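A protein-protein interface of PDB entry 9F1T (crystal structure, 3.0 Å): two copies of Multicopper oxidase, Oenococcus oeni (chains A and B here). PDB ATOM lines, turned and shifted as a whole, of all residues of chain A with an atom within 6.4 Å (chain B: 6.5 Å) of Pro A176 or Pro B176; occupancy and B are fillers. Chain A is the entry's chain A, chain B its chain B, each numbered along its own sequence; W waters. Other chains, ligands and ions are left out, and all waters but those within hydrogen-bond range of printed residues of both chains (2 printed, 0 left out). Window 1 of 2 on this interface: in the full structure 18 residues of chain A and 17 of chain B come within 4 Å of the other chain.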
ATOM      1  N   ASP A 174      -5.186  13.204 -24.978  1.00  0.00           N
ATOM      2  CA  ASP A 174      -6.482  13.749 -25.348  1.00  0.00           C
ATOM      3  C   ASP A 174      -6.948  14.721 -24.262  1.00  0.00           C
ATOM      4  O   ASP A 174      -6.601  14.559 -23.093  1.00  0.00           O
ATOM      5  CB  ASP A 174      -7.498  12.651 -25.622  1.00  0.00           C
ATOM      6  CG  ASP A 174      -8.902  13.126 -25.988  1.00  0.00           C
ATOM      7  OD1 ASP A 174      -9.010  14.042 -26.835  1.00  0.00           O
ATOM      8  OD2 ASP A 174      -9.883  12.573 -25.427  1.00  0.00           O
ATOM      9  N   LEU A 175      -7.730  15.731 -24.673  1.00  0.00           N
ATOM     10  CA  LEU A 175      -8.278  16.731 -23.769  1.00  0.00           C
ATOM     11  C   LEU A 175      -9.795  16.582 -23.712  1.00  0.00           C
ATOM     12  O   LEU A 175     -10.513  17.175 -24.515  1.00  0.00           O
ATOM     13  CB  LEU A 175      -7.882  18.130 -24.237  1.00  0.00           C
ATOM     14  CG  LEU A 175      -6.393  18.475 -24.127  1.00  0.00           C
ATOM     15  CD1 LEU A 175      -6.119  19.821 -24.780  1.00  0.00           C
ATOM     16  CD2 LEU A 175      -5.901  18.475 -22.680  1.00  0.00           C
ATOM     17  N   PRO A 176     -10.335  15.814 -22.739  1.00  0.00           N
ATOM     18  CA  PRO A 176     -11.772  15.539 -22.700  1.00  0.00           C
ATOM     19  C   PRO A 176     -12.618  16.693 -22.168  1.00  0.00           C
ATOM     20  O   PRO A 176     -13.819  16.526 -21.961  1.00  0.00           O
ATOM     21  CB  PRO A 176     -11.824  14.304 -21.792  1.00  0.00           C
ATOM     22  CG  PRO A 176     -10.703  14.532 -20.808  1.00  0.00           C
ATOM     23  CD  PRO A 176      -9.604  15.198 -21.620  1.00  0.00           C
ATOM     24  N   GLN A 177     -11.979  17.853 -21.960  1.00  0.00           N
ATOM     25  CA  GLN A 177     -12.670  19.087 -21.614  1.00  0.00           C
ATOM     26  C   GLN A 177     -13.302  19.698 -22.862  1.00  0.00           C
ATOM     27  O   GLN A 177     -14.250  20.466 -22.752  1.00  0.00           O
ATOM     28  CB  GLN A 177     -11.750  20.169 -21.043  1.00  0.00           C
ATOM     29  CG  GLN A 177     -10.997  19.765 -19.782  1.00  0.00           C
ATOM     30  CD  GLN A 177      -9.776  18.916 -20.058  1.00  0.00           C
ATOM     31  OE1 GLN A 177      -9.459  18.589 -21.208  1.00  0.00           O
ATOM     32  NE2 GLN A 177      -9.080  18.538 -18.998  1.00  0.00           N
ATOM     33  N   LEU A 178     -12.751  19.367 -24.033  1.00  0.00           N
ATOM     34  CA  LEU A 178     -13.210  19.931 -25.288  1.00  0.00           C
ATOM     35  C   LEU A 178     -14.547  19.307 -25.670  1.00  0.00           C
ATOM     36  O   LEU A 178     -14.824  18.154 -25.341  1.00  0.00           O
ATOM     37  CB  LEU A 178     -12.183  19.679 -26.389  1.00  0.00           C
ATOM     38  CG  LEU A 178     -10.759  20.168 -26.113  1.00  0.00           C
ATOM     39  CD1 LEU A 178      -9.828  19.783 -27.250  1.00  0.00           C
ATOM     40  CD2 LEU A 178     -10.751  21.661 -25.892  1.00  0.00           C
ATOM     41  N   PRO A 179     -15.415  20.069 -26.369  1.00  0.00           N
ATOM     42  CA  PRO A 179     -16.552  19.487 -27.080  1.00  0.00           C
ATOM     43  C   PRO A 179     -16.154  18.263 -27.901  1.00  0.00           C
ATOM     44  O   PRO A 179     -15.195  18.324 -28.674  1.00  0.00           O
ATOM     45  CB  PRO A 179     -16.980  20.665 -27.964  1.00  0.00           C
ATOM     46  CG  PRO A 179     -16.682  21.877 -27.116  1.00  0.00           C
ATOM     47  CD  PRO A 179     -15.369  21.536 -26.461  1.00  0.00           C
ATOM     48  N   HIS A 180     -16.883  17.153 -27.714  1.00  0.00           N
ATOM     49  CA  HIS A 180     -16.624  15.955 -28.494  1.00  0.00           C
ATOM     50  C   HIS A 180     -17.898  15.309 -29.033  1.00  0.00           C
ATOM     51  O   HIS A 180     -17.795  14.327 -29.761  1.00  0.00           O
ATOM     52  CB  HIS A 180     -15.766  14.958 -27.713  1.00  0.00           C
ATOM     53  CG  HIS A 180     -16.306  14.490 -26.404  1.00  0.00           C
ATOM     54  ND1 HIS A 180     -17.318  13.550 -26.345  1.00  0.00           N
ATOM     55  CD2 HIS A 180     -16.083  14.871 -25.139  1.00  0.00           C
ATOM     56  CE1 HIS A 180     -17.666  13.352 -25.078  1.00  0.00           C
ATOM     57  NE2 HIS A 180     -16.931  14.146 -24.331  1.00  0.00           N
ATOM     58  N   ARG A 322     -15.716  24.118 -20.239  1.00  0.00           N
ATOM     59  CA  ARG A 322     -14.879  23.556 -19.191  1.00  0.00           C
ATOM     60  C   ARG A 322     -13.523  24.259 -19.216  1.00  0.00           C
ATOM     61  O   ARG A 322     -12.925  24.428 -20.274  1.00  0.00           O
ATOM     62  CB  ARG A 322     -14.706  22.047 -19.401  1.00  0.00           C
ATOM     63  CG  ARG A 322     -15.986  21.228 -19.324  1.00  0.00           C
ATOM     64  CD  ARG A 322     -16.530  21.112 -17.907  1.00  0.00           C
ATOM     65  NE  ARG A 322     -17.737  20.281 -17.821  1.00  0.00           N
ATOM     66  CZ  ARG A 322     -18.947  20.618 -18.253  1.00  0.00           C
ATOM     67  NH1 ARG A 322     -19.147  21.787 -18.835  1.00  0.00           N
ATOM     68  NH2 ARG A 322     -19.961  19.789 -18.091  1.00  0.00           N
ATOM     69  N   ASP B 174     -17.114  20.065 -12.637  1.00  0.00           N
ATOM     70  CA  ASP B 174     -17.286  18.766 -13.268  1.00  0.00           C
ATOM     71  C   ASP B 174     -15.923  18.294 -13.763  1.00  0.00           C
ATOM     72  O   ASP B 174     -15.061  19.112 -14.083  1.00  0.00           O
ATOM     73  CB  ASP B 174     -18.330  18.793 -14.376  1.00  0.00           C
ATOM     74  CG  ASP B 174     -18.531  17.472 -15.117  1.00  0.00           C
ATOM     75  OD1 ASP B 174     -18.558  16.413 -14.441  1.00  0.00           O
ATOM     76  OD2 ASP B 174     -18.662  17.499 -16.366  1.00  0.00           O
ATOM     77  N   LEU B 175     -15.751  16.965 -13.793  1.00  0.00           N
ATOM     78  CA  LEU B 175     -14.523  16.336 -14.252  1.00  0.00           C
ATOM     79  C   LEU B 175     -14.807  15.579 -15.544  1.00  0.00           C
ATOM     80  O   LEU B 175     -15.243  14.431 -15.504  1.00  0.00           O
ATOM     81  CB  LEU B 175     -13.986  15.404 -13.167  1.00  0.00           C
ATOM     82  CG  LEU B 175     -13.507  16.090 -11.884  1.00  0.00           C
ATOM     83  CD1 LEU B 175     -13.240  15.070 -10.796  1.00  0.00           C
ATOM     84  CD2 LEU B 175     -12.266  16.948 -12.138  1.00  0.00           C
ATOM     85  N   PRO B 176     -14.554  16.189 -16.725  1.00  0.00           N
ATOM     86  CA  PRO B 176     -14.891  15.554 -17.997  1.00  0.00           C
ATOM     87  C   PRO B 176     -13.924  14.448 -18.422  1.00  0.00           C
ATOM     88  O   PRO B 176     -14.043  13.930 -19.529  1.00  0.00           O
ATOM     89  CB  PRO B 176     -14.879  16.760 -18.949  1.00  0.00           C
ATOM     90  CG  PRO B 176     -13.785  17.643 -18.403  1.00  0.00           C
ATOM     91  CD  PRO B 176     -13.920  17.506 -16.897  1.00  0.00           C
ATOM     92  N   GLN B 177     -12.989  14.090 -17.529  1.00  0.00           N
ATOM     93  CA  GLN B 177     -12.115  12.944 -17.713  1.00  0.00           C
ATOM     94  C   GLN B 177     -12.861  11.646 -17.419  1.00  0.00           C
ATOM     95  O   GLN B 177     -12.457  10.581 -17.877  1.00  0.00           O
ATOM     96  CB  GLN B 177     -10.906  12.963 -16.779  1.00  0.00           C
ATOM     97  CG  GLN B 177      -9.988  14.165 -16.972  1.00  0.00           C
ATOM     98  CD  GLN B 177     -10.474  15.415 -16.274  1.00  0.00           C
ATOM     99  OE1 GLN B 177     -11.555  15.453 -15.672  1.00  0.00           O
ATOM    100  NE2 GLN B 177      -9.656  16.454 -16.348  1.00  0.00           N
ATOM    101  N   LEU B 178     -13.932  11.742 -16.631  1.00  0.00           N
ATOM    102  CA  LEU B 178     -14.696  10.579 -16.214  1.00  0.00           C
ATOM    103  C   LEU B 178     -15.522  10.046 -17.381  1.00  0.00           C
ATOM    104  O   LEU B 178     -15.912  10.792 -18.274  1.00  0.00           O
ATOM    105  CB  LEU B 178     -15.597  10.951 -15.037  1.00  0.00           C
ATOM    106  CG  LEU B 178     -14.894  11.539 -13.810  1.00  0.00           C
ATOM    107  CD1 LEU B 178     -15.899  11.921 -12.751  1.00  0.00           C
ATOM    108  CD2 LEU B 178     -13.873  10.555 -13.255  1.00  0.00           C
ATOM    109  N   PRO B 179     -15.784   8.723 -17.413  1.00  0.00           N
ATOM    110  CA  PRO B 179     -16.870   8.165 -18.218  1.00  0.00           C
ATOM    111  C   PRO B 179     -18.174   8.931 -18.027  1.00  0.00           C
ATOM    112  O   PRO B 179     -18.605   9.123 -16.895  1.00  0.00           O
ATOM    113  CB  PRO B 179     -16.967   6.733 -17.675  1.00  0.00           C
ATOM    114  CG  PRO B 179     -15.554   6.399 -17.257  1.00  0.00           C
ATOM    115  CD  PRO B 179     -15.001   7.694 -16.710  1.00  0.00           C
ATOM    116  N   HIS B 180     -18.791   9.363 -19.134  1.00  0.00           N
ATOM    117  CA  HIS B 180     -20.045  10.099 -19.066  1.00  0.00           C
ATOM    118  C   HIS B 180     -21.063   9.589 -20.086  1.00  0.00           C
ATOM    119  O   HIS B 180     -22.194  10.054 -20.077  1.00  0.00           O
ATOM    120  CB  HIS B 180     -19.793  11.607 -19.218  1.00  0.00           C
ATOM    121  CG  HIS B 180     -19.337  12.043 -20.577  1.00  0.00           C
ATOM    122  ND1 HIS B 180     -18.011  11.991 -20.962  1.00  0.00           N
ATOM    123  CD2 HIS B 180     -20.012  12.530 -21.637  1.00  0.00           C
ATOM    124  CE1 HIS B 180     -17.899  12.431 -22.209  1.00  0.00           C
ATOM    125  NE2 HIS B 180     -19.101  12.770 -22.641  1.00  0.00           N
ATOM    126  N   ARG B 322      -8.584   8.256 -18.792  1.00  0.00           N
ATOM    127  CA  ARG B 322      -7.946   9.566 -18.823  1.00  0.00           C
ATOM    128  C   ARG B 322      -7.399   9.884 -17.432  1.00  0.00           C
ATOM    129  O   ARG B 322      -8.120   9.756 -16.447  1.00  0.00           O
ATOM    130  CB  ARG B 322      -8.965  10.646 -19.222  1.00  0.00           C
ATOM    131  CG  ARG B 322      -9.602  10.498 -20.597  1.00  0.00           C
ATOM    132  CD  ARG B 322      -8.639  10.839 -21.728  1.00  0.00           C
ATOM    133  NE  ARG B 322      -9.268  10.750 -23.052  1.00  0.00           N
ATOM    134  CZ  ARG B 322      -9.593   9.613 -23.674  1.00  0.00           C
ATOM    135  NH1 ARG B 322      -9.326   8.435 -23.129  1.00  0.00           N
ATOM    136  NH2 ARG B 322     -10.173   9.646 -24.861  1.00  0.00           N
HETATM  137  O   HOH W   1      -6.683  16.634 -18.047  1.00  0.00           O
HETATM  138  O   HOH W   2     -18.879  15.833 -22.492  1.00  0.00           O
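Water W2 lies within hydrogen-bond range of NE2 of His B180 (3.1 Å) and NE2 of His A180 (3.2 Å).
Water W1 lies within hydrogen-bond range of the side-chain amide nitrogen (NE2) of Gln A177 and the side-chain amide nitrogen (NE2) of Gln B177.
Asp A174 touches Arg B322, and with the chains exchanged Arg A322 touches Asp B174.
Pro B176 touches its own counterpart, Pro A176.
Gln B177 touches its own counterpart, Gln A177.
His A180 touches its own counterpart, His B180.
Positions printed for both chains: 174, 175, 176, 177, 178, 179, 180 and 322.
Of the 7 pairs that touch across the chains among the printed residues, 7 have their exchanged pair printed and touching as well.
Of the 8 printed residues of chain B, 5 touch a printed residue of chain A.
Hydrophobic or aromatic side chains of chain B within 4 Å of the printed part of chain A: Pro B176 and His B180.
Along chain B the printed residues that touch a printed residue of chain A span positions 174 to 322.
Printed residues of chain A that touch a printed residue of chain B: Asp A174, Pro A176, Gln A177, His A180 and Arg A322.
Among the printed residues, 7 pairs touch across the chains.
The guanidinium group (NH2) of Arg A322 is in salt-bridge range of the side-chain carboxylate (OD2) of Asp B174 (3.1 Å).
NE2 of Gln A177 sits close to NE2 of Gln B177 (3.4 Å).
A ring nitrogen (NE2) of His A180 sits close to a ring nitrogen (NE2) of His B180.
The guanidinium group (NH2) of Arg B322 is in salt-bridge range of the side-chain carboxylate (OD2) of Asp A174 (3.0 Å).
Printed residues of chain B within 4 Å of Pro A176: Pro B176 and Gln B177.
Printed residues of chain B within 4 Å of Gln A177: Pro B176 (3.7 Å) and Gln B177 (3.4 Å).
Printed residues of chain B within 4 Å of Arg A322: Asp B174.
Of the printed residues of chain A, Asp B174 touches Arg A322 (3.1 Å).
Of the printed residues of chain A, Pro B176 touches Pro A176 and Gln A177.
Leu B178 touches none of the printed residues of chain A.
Of the printed residues of chain A, His B180 touches His A180.
The nearest residue of chain A that does not touch Pro B176 is Arg A322 (4.3 Å).
Among the printed residues, merely in contact across the chains: Pro A176 with Pro B176 (3.2 Å), Gln A177 with Pro B176 (3.7 Å) and Pro A176 with Gln B177 (3.8 Å).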
